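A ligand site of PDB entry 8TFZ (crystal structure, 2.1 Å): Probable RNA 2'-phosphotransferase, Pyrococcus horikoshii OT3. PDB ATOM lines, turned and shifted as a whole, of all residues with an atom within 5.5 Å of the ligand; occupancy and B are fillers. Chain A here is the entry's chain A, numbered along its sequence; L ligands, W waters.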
ATOM      1  N   ARG A  62     -17.823  19.864 -30.500  1.00  0.00           N
ATOM      2  CA  ARG A  62     -17.630  21.190 -29.955  1.00  0.00           C
ATOM      3  C   ARG A  62     -18.931  21.987 -29.863  1.00  0.00           C
ATOM      4  O   ARG A  62     -18.986  22.984 -29.121  1.00  0.00           O
ATOM      5  CB  ARG A  62     -16.627  21.910 -30.846  1.00  0.00           C
ATOM      6  CG  ARG A  62     -16.628  23.423 -30.725  1.00  0.00           C
ATOM      7  CD  ARG A  62     -15.775  23.812 -29.539  1.00  0.00           C
ATOM      8  NE  ARG A  62     -15.783  25.225 -29.222  1.00  0.00           N
ATOM      9  CZ  ARG A  62     -14.737  26.015 -29.366  1.00  0.00           C
ATOM     10  NH1 ARG A  62     -13.583  25.553 -29.853  1.00  0.00           N
ATOM     11  NH2 ARG A  62     -14.826  27.283 -28.996  1.00  0.00           N
ATOM     12  N   TYR A  74     -17.667  24.728 -25.325  1.00  0.00           N
ATOM     13  CA  TYR A  74     -16.463  25.116 -24.599  1.00  0.00           C
ATOM     14  C   TYR A  74     -15.636  26.090 -25.437  1.00  0.00           C
ATOM     15  O   TYR A  74     -15.877  26.256 -26.630  1.00  0.00           O
ATOM     16  CB  TYR A  74     -15.629  23.887 -24.230  1.00  0.00           C
ATOM     17  CG  TYR A  74     -15.063  23.117 -25.417  1.00  0.00           C
ATOM     18  CD1 TYR A  74     -13.859  23.493 -26.018  1.00  0.00           C
ATOM     19  CD2 TYR A  74     -15.738  22.016 -25.933  1.00  0.00           C
ATOM     20  CE1 TYR A  74     -13.327  22.769 -27.103  1.00  0.00           C
ATOM     21  CE2 TYR A  74     -15.245  21.323 -27.017  1.00  0.00           C
ATOM     22  CZ  TYR A  74     -14.037  21.690 -27.597  1.00  0.00           C
ATOM     23  OH  TYR A  74     -13.538  20.937 -28.678  1.00  0.00           O
ATOM     24  N   GLY A  75     -14.647  26.709 -24.795  1.00  0.00           N
ATOM     25  CA  GLY A  75     -13.725  27.577 -25.485  1.00  0.00           C
ATOM     26  C   GLY A  75     -14.195  28.998 -25.743  1.00  0.00           C
ATOM     27  O   GLY A  75     -13.500  29.734 -26.448  1.00  0.00           O
ATOM     28  N   TYR A  94      -3.479  15.375 -21.677  1.00  0.00           N
ATOM     29  CA  TYR A  94      -2.379  16.106 -22.285  1.00  0.00           C
ATOM     30  C   TYR A  94      -2.689  17.585 -22.348  1.00  0.00           C
ATOM     31  O   TYR A  94      -3.849  17.977 -22.540  1.00  0.00           O
ATOM     32  CB  TYR A  94      -2.052  15.580 -23.664  1.00  0.00           C
ATOM     33  CG  TYR A  94      -1.743  14.108 -23.712  1.00  0.00           C
ATOM     34  CD1 TYR A  94      -0.438  13.638 -23.619  1.00  0.00           C
ATOM     35  CD2 TYR A  94      -2.772  13.169 -23.904  1.00  0.00           C
ATOM     36  CE1 TYR A  94      -0.163  12.240 -23.697  1.00  0.00           C
ATOM     37  CE2 TYR A  94      -2.500  11.791 -23.963  1.00  0.00           C
ATOM     38  CZ  TYR A  94      -1.198  11.341 -23.850  1.00  0.00           C
ATOM     39  OH  TYR A  94      -0.941   9.980 -23.909  1.00  0.00           O
ATOM     40  N   HIS A  95      -1.675  18.416 -22.160  1.00  0.00           N
ATOM     41  CA  HIS A  95      -1.834  19.870 -22.345  1.00  0.00           C
ATOM     42  C   HIS A  95      -0.748  20.372 -23.283  1.00  0.00           C
ATOM     43  O   HIS A  95       0.436  20.247 -22.974  1.00  0.00           O
ATOM     44  CB  HIS A  95      -1.748  20.618 -21.021  1.00  0.00           C
ATOM     45  CG  HIS A  95      -1.862  22.116 -21.151  1.00  0.00           C
ATOM     46  ND1 HIS A  95      -3.051  22.758 -21.403  1.00  0.00           N
ATOM     47  CD2 HIS A  95      -0.932  23.089 -21.033  1.00  0.00           C
ATOM     48  CE1 HIS A  95      -2.858  24.070 -21.440  1.00  0.00           C
ATOM     49  NE2 HIS A  95      -1.577  24.301 -21.196  1.00  0.00           N
ATOM     50  N   GLY A  96      -1.139  20.986 -24.394  1.00  0.00           N
ATOM     51  CA  GLY A  96      -0.177  21.465 -25.390  1.00  0.00           C
ATOM     52  C   GLY A  96       0.064  22.942 -25.127  1.00  0.00           C
ATOM     53  O   GLY A  96      -0.892  23.679 -24.851  1.00  0.00           O
ATOM     54  N   THR A  97       1.333  23.348 -25.182  1.00  0.00           N
ATOM     55  CA  THR A  97       1.739  24.733 -24.959  1.00  0.00           C
ATOM     56  C   THR A  97       3.040  24.955 -25.721  1.00  0.00           C
ATOM     57  O   THR A  97       3.513  24.080 -26.433  1.00  0.00           O
ATOM     58  CB  THR A  97       1.902  25.020 -23.449  1.00  0.00           C
ATOM     59  OG1 THR A  97       2.010  26.430 -23.232  1.00  0.00           O
ATOM     60  CG2 THR A  97       3.114  24.331 -22.865  1.00  0.00           C
ATOM     61  N   VAL A  98       3.616  26.165 -25.615  1.00  0.00           N
ATOM     62  CA  VAL A  98       4.903  26.429 -26.197  1.00  0.00           C
ATOM     63  C   VAL A  98       5.959  26.445 -25.100  1.00  0.00           C
ATOM     64  O   VAL A  98       5.675  26.658 -23.911  1.00  0.00           O
ATOM     65  CB  VAL A  98       4.931  27.731 -27.003  1.00  0.00           C
ATOM     66  CG1 VAL A  98       4.370  27.447 -28.329  1.00  0.00           C
ATOM     67  CG2 VAL A  98       4.156  28.816 -26.275  1.00  0.00           C
ATOM     68  N   ASN A 101       6.587  28.734 -22.044  1.00  0.00           N
ATOM     69  CA  ASN A 101       5.688  28.659 -20.901  1.00  0.00           C
ATOM     70  C   ASN A 101       6.112  27.627 -19.844  1.00  0.00           C
ATOM     71  O   ASN A 101       5.547  27.650 -18.743  1.00  0.00           O
ATOM     72  CB  ASN A 101       4.280  28.347 -21.391  1.00  0.00           C
ATOM     73  CG  ASN A 101       3.672  29.494 -22.107  1.00  0.00           C
ATOM     74  OD1 ASN A 101       4.061  30.637 -21.861  1.00  0.00           O
ATOM     75  ND2 ASN A 101       2.723  29.221 -23.010  1.00  0.00           N
ATOM     76  N   GLY A 104       7.013  29.046 -16.419  1.00  0.00           N
ATOM     77  CA  GLY A 104       5.884  29.389 -15.567  1.00  0.00           C
ATOM     78  C   GLY A 104       5.239  28.136 -14.992  1.00  0.00           C
ATOM     79  O   GLY A 104       5.070  27.997 -13.776  1.00  0.00           O
ATOM     80  N   ILE A 105       4.995  27.160 -15.871  1.00  0.00           N
ATOM     81  CA  ILE A 105       4.188  26.014 -15.509  1.00  0.00           C
ATOM     82  C   ILE A 105       4.890  25.191 -14.445  1.00  0.00           C
ATOM     83  O   ILE A 105       4.312  24.888 -13.388  1.00  0.00           O
ATOM     84  CB  ILE A 105       3.835  25.197 -16.768  1.00  0.00           C
ATOM     85  CG1 ILE A 105       2.931  26.064 -17.657  1.00  0.00           C
ATOM     86  CG2 ILE A 105       3.252  23.884 -16.367  1.00  0.00           C
ATOM     87  CD1 ILE A 105       2.253  25.431 -18.876  1.00  0.00           C
ATOM     88  N   GLU A 108       4.433  27.012 -11.196  1.00  0.00           N
ATOM     89  CA  GLU A 108       3.106  27.487 -10.856  1.00  0.00           C
ATOM     90  C   GLU A 108       2.052  26.426 -11.100  1.00  0.00           C
ATOM     91  O   GLU A 108       0.969  26.496 -10.511  1.00  0.00           O
ATOM     92  CB  GLU A 108       2.771  28.733 -11.700  1.00  0.00           C
ATOM     93  CG  GLU A 108       3.352  29.976 -11.133  1.00  0.00           C
ATOM     94  CD  GLU A 108       2.463  31.195 -11.326  1.00  0.00           C
ATOM     95  OE1 GLU A 108       1.242  31.034 -11.508  1.00  0.00           O
ATOM     96  OE2 GLU A 108       2.984  32.351 -11.182  1.00  0.00           O
ATOM     97  N   GLY A 109       2.376  25.416 -11.894  1.00  0.00           N
ATOM     98  CA  GLY A 109       1.370  24.507 -12.411  1.00  0.00           C
ATOM     99  C   GLY A 109       0.703  25.161 -13.581  1.00  0.00           C
ATOM    100  O   GLY A 109       1.015  26.289 -13.961  1.00  0.00           O
ATOM    101  N   ILE A 110      -0.247  24.451 -14.172  1.00  0.00           N
ATOM    102  CA  ILE A 110      -0.998  25.001 -15.300  1.00  0.00           C
ATOM    103  C   ILE A 110      -2.182  25.798 -14.755  1.00  0.00           C
ATOM    104  O   ILE A 110      -3.009  25.266 -14.009  1.00  0.00           O
ATOM    105  CB  ILE A 110      -1.454  23.895 -16.255  1.00  0.00           C
ATOM    106  CG1 ILE A 110      -0.372  22.781 -16.354  1.00  0.00           C
ATOM    107  CG2 ILE A 110      -1.712  24.466 -17.606  1.00  0.00           C
ATOM    108  CD1 ILE A 110      -0.689  21.741 -17.414  1.00  0.00           C
ATOM    109  N   LYS A 111      -2.263  27.040 -15.128  1.00  0.00           N
ATOM    110  CA  LYS A 111      -3.381  27.812 -14.608  1.00  0.00           C
ATOM    111  C   LYS A 111      -4.347  28.203 -15.711  1.00  0.00           C
ATOM    112  O   LYS A 111      -3.967  28.264 -16.891  1.00  0.00           O
ATOM    113  CB  LYS A 111      -2.883  29.069 -13.884  1.00  0.00           C
ATOM    114  CG  LYS A 111      -1.836  29.834 -14.630  1.00  0.00           C
ATOM    115  CD  LYS A 111      -1.532  31.163 -13.894  1.00  0.00           C
ATOM    116  CE  LYS A 111      -0.497  32.019 -14.623  1.00  0.00           C
ATOM    117  NZ  LYS A 111       0.191  32.990 -13.671  1.00  0.00           N
ATOM    118  N   PRO A 112      -5.618  28.424 -15.374  1.00  0.00           N
ATOM    119  CA  PRO A 112      -6.623  28.712 -16.408  1.00  0.00           C
ATOM    120  C   PRO A 112      -6.501  30.115 -17.046  1.00  0.00           C
ATOM    121  O   PRO A 112      -7.152  30.363 -18.068  1.00  0.00           O
ATOM    122  CB  PRO A 112      -7.945  28.568 -15.648  1.00  0.00           C
ATOM    123  CG  PRO A 112      -7.596  28.859 -14.244  1.00  0.00           C
ATOM    124  CD  PRO A 112      -6.233  28.283 -14.050  1.00  0.00           C
ATOM    125  N   ARG A 115      -9.660  31.982 -18.687  1.00  0.00           N
ATOM    126  CA  ARG A 115     -10.831  31.123 -18.740  1.00  0.00           C
ATOM    127  C   ARG A 115     -11.204  30.634 -17.360  1.00  0.00           C
ATOM    128  O   ARG A 115     -10.464  30.812 -16.405  1.00  0.00           O
ATOM    129  CB  ARG A 115     -10.571  29.918 -19.640  1.00  0.00           C
ATOM    130  CG  ARG A 115      -9.954  30.298 -20.944  1.00  0.00           C
ATOM    131  CD  ARG A 115      -9.614  29.054 -21.769  1.00  0.00           C
ATOM    132  NE  ARG A 115      -8.992  29.519 -22.998  1.00  0.00           N
ATOM    133  CZ  ARG A 115      -9.707  29.884 -24.050  1.00  0.00           C
ATOM    134  NH1 ARG A 115     -11.007  29.674 -24.102  1.00  0.00           N
ATOM    135  NH2 ARG A 115      -9.085  30.457 -25.093  1.00  0.00           N
ATOM    136  N   HIS A 119      -7.667  23.638 -20.153  1.00  0.00           N
ATOM    137  CA  HIS A 119      -8.110  22.730 -21.189  1.00  0.00           C
ATOM    138  C   HIS A 119      -7.044  21.680 -21.491  1.00  0.00           C
ATOM    139  O   HIS A 119      -5.866  22.017 -21.715  1.00  0.00           O
ATOM    140  CB  HIS A 119      -8.487  23.563 -22.412  1.00  0.00           C
ATOM    141  CG  HIS A 119      -9.710  24.394 -22.177  1.00  0.00           C
ATOM    142  ND1 HIS A 119     -10.821  24.339 -22.986  1.00  0.00           N
ATOM    143  CD2 HIS A 119     -10.032  25.243 -21.165  1.00  0.00           C
ATOM    144  CE1 HIS A 119     -11.751  25.160 -22.535  1.00  0.00           C
ATOM    145  NE2 HIS A 119     -11.303  25.719 -21.423  1.00  0.00           N
ATOM    146  N   LEU A 120      -7.432  20.410 -21.429  1.00  0.00           N
ATOM    147  CA  LEU A 120      -6.620  19.212 -21.653  1.00  0.00           C
ATOM    148  C   LEU A 120      -7.193  18.432 -22.824  1.00  0.00           C
ATOM    149  O   LEU A 120      -8.323  18.660 -23.273  1.00  0.00           O
ATOM    150  CB  LEU A 120      -6.616  18.301 -20.415  1.00  0.00           C
ATOM    151  CG  LEU A 120      -6.150  19.045 -19.153  1.00  0.00           C
ATOM    152  CD1 LEU A 120      -6.496  18.280 -17.923  1.00  0.00           C
ATOM    153  CD2 LEU A 120      -4.626  19.373 -19.255  1.00  0.00           C
ATOM    154  N   SER A 121      -6.450  17.478 -23.314  1.00  0.00           N
ATOM    155  CA  SER A 121      -6.990  16.627 -24.345  1.00  0.00           C
ATOM    156  C   SER A 121      -6.692  15.173 -24.011  1.00  0.00           C
ATOM    157  O   SER A 121      -5.670  14.868 -23.389  1.00  0.00           O
ATOM    158  CB  SER A 121      -6.428  17.032 -25.716  1.00  0.00           C
ATOM    159  OG  SER A 121      -6.386  15.895 -26.541  1.00  0.00           O
ATOM    160  N   ASP A 126      -4.306  16.217 -30.387  1.00  0.00           N
ATOM    161  CA  ASP A 126      -5.132  17.390 -30.171  1.00  0.00           C
ATOM    162  C   ASP A 126      -4.428  18.425 -29.314  1.00  0.00           C
ATOM    163  O   ASP A 126      -4.499  19.620 -29.604  1.00  0.00           O
ATOM    164  CB  ASP A 126      -6.449  16.997 -29.500  1.00  0.00           C
ATOM    165  CG  ASP A 126      -7.430  16.507 -30.460  1.00  0.00           C
ATOM    166  OD1 ASP A 126      -7.117  15.528 -31.164  1.00  0.00           O
ATOM    167  OD2 ASP A 126      -8.501  17.142 -30.581  1.00  0.00           O
ATOM    168  N   ALA A 127      -3.776  18.003 -28.213  1.00  0.00           N
ATOM    169  CA  ALA A 127      -3.080  18.972 -27.402  1.00  0.00           C
ATOM    170  C   ALA A 127      -2.022  19.708 -28.218  1.00  0.00           C
ATOM    171  O   ALA A 127      -1.884  20.927 -28.096  1.00  0.00           O
ATOM    172  CB  ALA A 127      -2.464  18.338 -26.169  1.00  0.00           C
ATOM    173  N   THR A 130      -3.591  22.268 -30.547  1.00  0.00           N
ATOM    174  CA  THR A 130      -4.063  23.454 -29.849  1.00  0.00           C
ATOM    175  C   THR A 130      -2.910  24.278 -29.321  1.00  0.00           C
ATOM    176  O   THR A 130      -3.012  25.515 -29.279  1.00  0.00           O
ATOM    177  CB  THR A 130      -4.990  23.092 -28.700  1.00  0.00           C
ATOM    178  OG1 THR A 130      -4.270  22.259 -27.797  1.00  0.00           O
ATOM    179  CG2 THR A 130      -6.208  22.334 -29.186  1.00  0.00           C
ATOM    180  N   GLY A 131      -1.825  23.624 -28.889  1.00  0.00           N
ATOM    181  CA  GLY A 131      -0.676  24.344 -28.365  1.00  0.00           C
ATOM    182  C   GLY A 131       0.018  25.153 -29.425  1.00  0.00           C
ATOM    183  O   GLY A 131       0.672  26.141 -29.104  1.00  0.00           O
ATOM    184  N   ARG A 133      -1.385  27.143 -31.470  1.00  0.00           N
ATOM    185  CA  ARG A 133      -1.926  28.498 -31.578  1.00  0.00           C
ATOM    186  C   ARG A 133      -0.949  29.555 -31.056  1.00  0.00           C
ATOM    187  O   ARG A 133      -0.949  30.692 -31.521  1.00  0.00           O
ATOM    188  CB  ARG A 133      -3.268  28.574 -30.856  1.00  0.00           C
ATOM    189  CG  ARG A 133      -4.417  27.910 -31.664  1.00  0.00           C
ATOM    190  CD  ARG A 133      -5.711  27.545 -30.886  1.00  0.00           C
ATOM    191  NE  ARG A 133      -6.456  28.686 -30.344  1.00  0.00           N
ATOM    192  CZ  ARG A 133      -7.278  29.466 -31.045  1.00  0.00           C
ATOM    193  NH1 ARG A 133      -7.415  29.346 -32.364  1.00  0.00           N
ATOM    194  NH2 ARG A 133      -7.978  30.424 -30.418  1.00  0.00           N
ATOM    195  N   HIS A 134      -0.060  29.191 -30.139  1.00  0.00           N
ATOM    196  CA  HIS A 134       0.804  30.170 -29.503  1.00  0.00           C
ATOM    197  C   HIS A 134       2.218  30.199 -30.045  1.00  0.00           C
ATOM    198  O   HIS A 134       3.061  30.941 -29.517  1.00  0.00           O
ATOM    199  CB  HIS A 134       0.840  29.947 -27.999  1.00  0.00           C
ATOM    200  CG  HIS A 134      -0.486  30.087 -27.372  1.00  0.00           C
ATOM    201  ND1 HIS A 134      -1.044  31.323 -27.102  1.00  0.00           N
ATOM    202  CD2 HIS A 134      -1.401  29.162 -26.992  1.00  0.00           C
ATOM    203  CE1 HIS A 134      -2.243  31.143 -26.571  1.00  0.00           C
ATOM    204  NE2 HIS A 134      -2.488  29.849 -26.491  1.00  0.00           N
ATOM    205  N   VAL A 162     -11.850  16.927 -25.599  1.00  0.00           N
ATOM    206  CA  VAL A 162     -11.422  18.023 -24.742  1.00  0.00           C
ATOM    207  C   VAL A 162     -11.849  17.717 -23.316  1.00  0.00           C
ATOM    208  O   VAL A 162     -13.007  17.385 -23.093  1.00  0.00           O
ATOM    209  CB  VAL A 162     -12.025  19.352 -25.235  1.00  0.00           C
ATOM    210  CG1 VAL A 162     -11.976  20.394 -24.153  1.00  0.00           C
ATOM    211  CG2 VAL A 162     -11.281  19.776 -26.493  1.00  0.00           C
ATOM    212  N   ARG A 163     -10.939  17.846 -22.353  1.00  0.00           N
ATOM    213  CA  ARG A 163     -11.282  17.770 -20.935  1.00  0.00           C
ATOM    214  C   ARG A 163     -10.897  19.058 -20.223  1.00  0.00           C
ATOM    215  O   ARG A 163      -9.928  19.709 -20.575  1.00  0.00           O
ATOM    216  CB  ARG A 163     -10.595  16.551 -20.242  1.00  0.00           C
ATOM    217  CG  ARG A 163     -10.901  15.212 -20.918  1.00  0.00           C
ATOM    218  CD  ARG A 163     -12.277  14.672 -20.507  1.00  0.00           C
ATOM    219  NE  ARG A 163     -12.684  13.441 -21.179  1.00  0.00           N
ATOM    220  CZ  ARG A 163     -13.224  13.393 -22.397  1.00  0.00           C
ATOM    221  NH1 ARG A 163     -13.341  14.482 -23.141  1.00  0.00           N
ATOM    222  NH2 ARG A 163     -13.651  12.234 -22.870  1.00  0.00           N
HETATM  223  P1  LIG L   1      -5.464  29.716 -23.885  1.00  0.00           P
HETATM  224  O1  LIG L   1      -5.486  29.891 -25.378  1.00  0.00           O
HETATM  225  O2  LIG L   1      -6.471  30.361 -22.987  1.00  0.00           O
HETATM  226  O3  LIG L   1      -4.011  30.102 -23.381  1.00  0.00           O
HETATM  227  C1  LIG L   1      -3.573  29.961 -22.015  1.00  0.00           C
HETATM  228  C2  LIG L   1      -2.105  29.663 -22.124  1.00  0.00           C
HETATM  229  O4  LIG L   1      -1.440  29.849 -20.852  1.00  0.00           O
HETATM  230  C3  LIG L   1      -1.755  28.234 -22.599  1.00  0.00           C
HETATM  231  O5  LIG L   1      -0.789  28.288 -23.637  1.00  0.00           O
HETATM  232  C4  LIG L   1      -1.139  27.610 -21.346  1.00  0.00           C
HETATM  233  O6  LIG L   1      -0.243  26.547 -21.613  1.00  0.00           O
HETATM  234  C5  LIG L   1      -0.476  28.834 -20.725  1.00  0.00           C
HETATM  235  N1  LIG L   1      -0.203  28.661 -19.323  1.00  0.00           N
HETATM  236  C6  LIG L   1      -0.939  27.909 -18.433  1.00  0.00           C
HETATM  237  N2  LIG L   1      -0.455  27.932 -17.229  1.00  0.00           N
HETATM  238  C7  LIG L   1       0.663  28.743 -17.320  1.00  0.00           C
HETATM  239  C8  LIG L   1       1.603  29.149 -16.363  1.00  0.00           C
HETATM  240  N3  LIG L   1       1.544  28.771 -15.095  1.00  0.00           N
HETATM  241  N4  LIG L   1       2.592  29.979 -16.775  1.00  0.00           N
HETATM  242  C9  LIG L   1       2.618  30.358 -18.071  1.00  0.00           C
HETATM  243  N5  LIG L   1       1.786  30.042 -19.062  1.00  0.00           N
HETATM  244  C10 LIG L   1       0.820  29.218 -18.611  1.00  0.00           C
HETATM  245  O7  LIG L   1      -5.491  28.143 -23.598  1.00  0.00           O
HETATM  246  P2  LIG L   1      -5.059  26.960 -24.594  1.00  0.00           P
HETATM  247  O8  LIG L   1      -5.287  25.676 -23.873  1.00  0.00           O
HETATM  248  O9  LIG L   1      -3.731  27.349 -25.165  1.00  0.00           O
HETATM  249  O10 LIG L   1      -6.147  27.121 -25.756  1.00  0.00           O
HETATM  250  C11 LIG L   1      -7.507  27.071 -25.349  1.00  0.00           C
HETATM  251  C12 LIG L   1      -8.344  26.594 -26.513  1.00  0.00           C
HETATM  252  O11 LIG L   1      -7.756  25.381 -27.048  1.00  0.00           O
HETATM  253  C13 LIG L   1      -9.778  26.224 -26.124  1.00  0.00           C
HETATM  254  O12 LIG L   1     -10.681  26.426 -27.193  1.00  0.00           O
HETATM  255  C14 LIG L   1      -9.614  24.757 -25.718  1.00  0.00           C
HETATM  256  O13 LIG L   1     -10.771  23.933 -25.744  1.00  0.00           O
HETATM  257  C15 LIG L   1      -8.598  24.266 -26.745  1.00  0.00           C
HETATM  258  N6  LIG L   1      -7.828  23.106 -26.213  1.00  0.00           N
HETATM  259  C16 LIG L   1      -6.511  23.227 -25.786  1.00  0.00           C
HETATM  260  C17 LIG L   1      -5.848  22.099 -25.317  1.00  0.00           C
HETATM  261  C18 LIG L   1      -4.405  22.139 -24.877  1.00  0.00           C
HETATM  262  O14 LIG L   1      -3.812  21.082 -24.616  1.00  0.00           O
HETATM  263  N7  LIG L   1      -3.820  23.321 -24.750  1.00  0.00           N
HETATM  264  C19 LIG L   1      -6.517  20.891 -25.195  1.00  0.00           C
HETATM  265  C20 LIG L   1      -7.826  20.783 -25.613  1.00  0.00           C
HETATM  266  C21 LIG L   1      -8.467  21.895 -26.113  1.00  0.00           C
HETATM  267  O   HOH W   1      -1.358  26.187 -25.139  1.00  0.00           O
HETATM  268  O   HOH W   2      -5.954  25.898 -21.125  1.00  0.00           O
HETATM  269  O   HOH W   3     -11.127  29.124 -27.512  1.00  0.00           O
HETATM  270  O   HOH W   4      -3.882  26.929 -19.548  1.00  0.00           O
HETATM  271  O   HOH W   5      -4.421  27.544 -27.930  1.00  0.00           O
HETATM  272  O   HOH W   6      -2.782  30.334 -18.261  1.00  0.00           O
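Water W1 lies within hydrogen-bond range of O of Gly 96 and O9 of the ligand.
Water W3 lies within hydrogen-bond range of the backbone carbonyl oxygen of Gly 75 (2.7 Å), an oxygen (O12) of the ligand (2.8 Å) and the guanidinium group of Arg 115 (3.4 Å).
Water W5 lies within hydrogen-bond range of an oxygen (O10) of the ligand, the backbone carbonyl oxygen of Thr 130, a ring nitrogen (NE2) of His 134 and the guanidinium group of Arg 133.
Water W2 lies within hydrogen-bond range of O8 of the ligand and N of His 119.
Water W6 bridges the backbone carbonyl oxygen (O) of Lys 111 (2.8 Å) and an oxygen (O4) of the ligand (3.0 Å).
O6 of the ligand is in hydrogen-bond range of NE2 of His 95, 2.6 Å away.
The guanidinium group (NE) of Arg 115 is in salt-bridge range of an oxygen (O2) of the ligand, at 2.7 Å.
O14 of the ligand sits at hydrogen-bond distance from N of Gly 96 (2.7 Å).
A nitrogen (N7) of the ligand lies within hydrogen-bond range of the backbone carbonyl oxygen (O) of Gly 96 (3.0 Å).
O6 of the ligand lies within hydrogen-bond range of OG1 of Thr 97 (2.8 Å).
O of Gly 109 is in hydrogen-bond range of N3 of the ligand, 2.8 Å away.
ND1 of His 119 lies within hydrogen-bond range of O13 of the ligand (2.8 Å).
The backbone NH (N) of Lys 111 is in hydrogen-bond range of a nitrogen (N2) of the ligand (2.9 Å).
OG1 of Thr 130 lies close to N7 of the ligand, 3.3 Å away.
NE2 of His 134 lies within hydrogen-bond range of O9 of the ligand (3.1 Å).
Tyr 74 touches the ligand.
CA of Gly 75 touches O12 of the ligand (3.7 Å).
Tyr 94 touches the ligand (O to O14, 3.7 Å).
Asn 101 touches the ligand (CG to N5, 3.6 Å).
Gly 104 touches the ligand (CA to N4, 3.6 Å).
Ile 105 touches the ligand.
Glu 108 touches the ligand.
CA of Ile 110 touches N2 of the ligand, at 3.6 Å.
O of Leu 120 touches C20 of the ligand (3.2 Å).
CB of Ser 121 touches C19 of the ligand, 3.9 Å away.
Ala 127 touches the ligand (CB to O14, 3.4 Å).
Val 162 touches the ligand.
Hydrophobic or aromatic side chains within 4 Å of the ligand: Tyr 74, His 95, Ile 105, Ile 110, His 119, Ala 127, His 134 and Val 162.
Of the 28 residues printed, 21 come within 4 Å of the ligand.
A ring nitrogen (ND1) of His 95 sits at hydrogen-bond distance from the backbone carbonyl oxygen of His 119 (2.9 Å).
NH1 of Arg 115 sits at hydrogen-bond distance from O of Gly 75 (3.4 Å).
ND2 of Asn 101 sits at hydrogen-bond distance from OG1 of Thr 97 (2.9 Å).
OE1 of Glu 108 is in salt-bridge range of NZ of Lys 111.
The side-chain hydroxyl (OG1) of Thr 130 sits at hydrogen-bond distance from the backbone carbonyl oxygen (O) of Ala 127 (2.7 Å).
OG1 of Thr 130 is in hydrogen-bond range of O of Asp 126, 3.2 Å away.
The backbone carbonyl oxygen (O) of Arg 163 is in hydrogen-bond range of the backbone NH (N) of Leu 120 (2.7 Å).
The backbone NH (N) of Ser 121 is in hydrogen-bond range of the backbone carbonyl oxygen (O) of Tyr 94.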
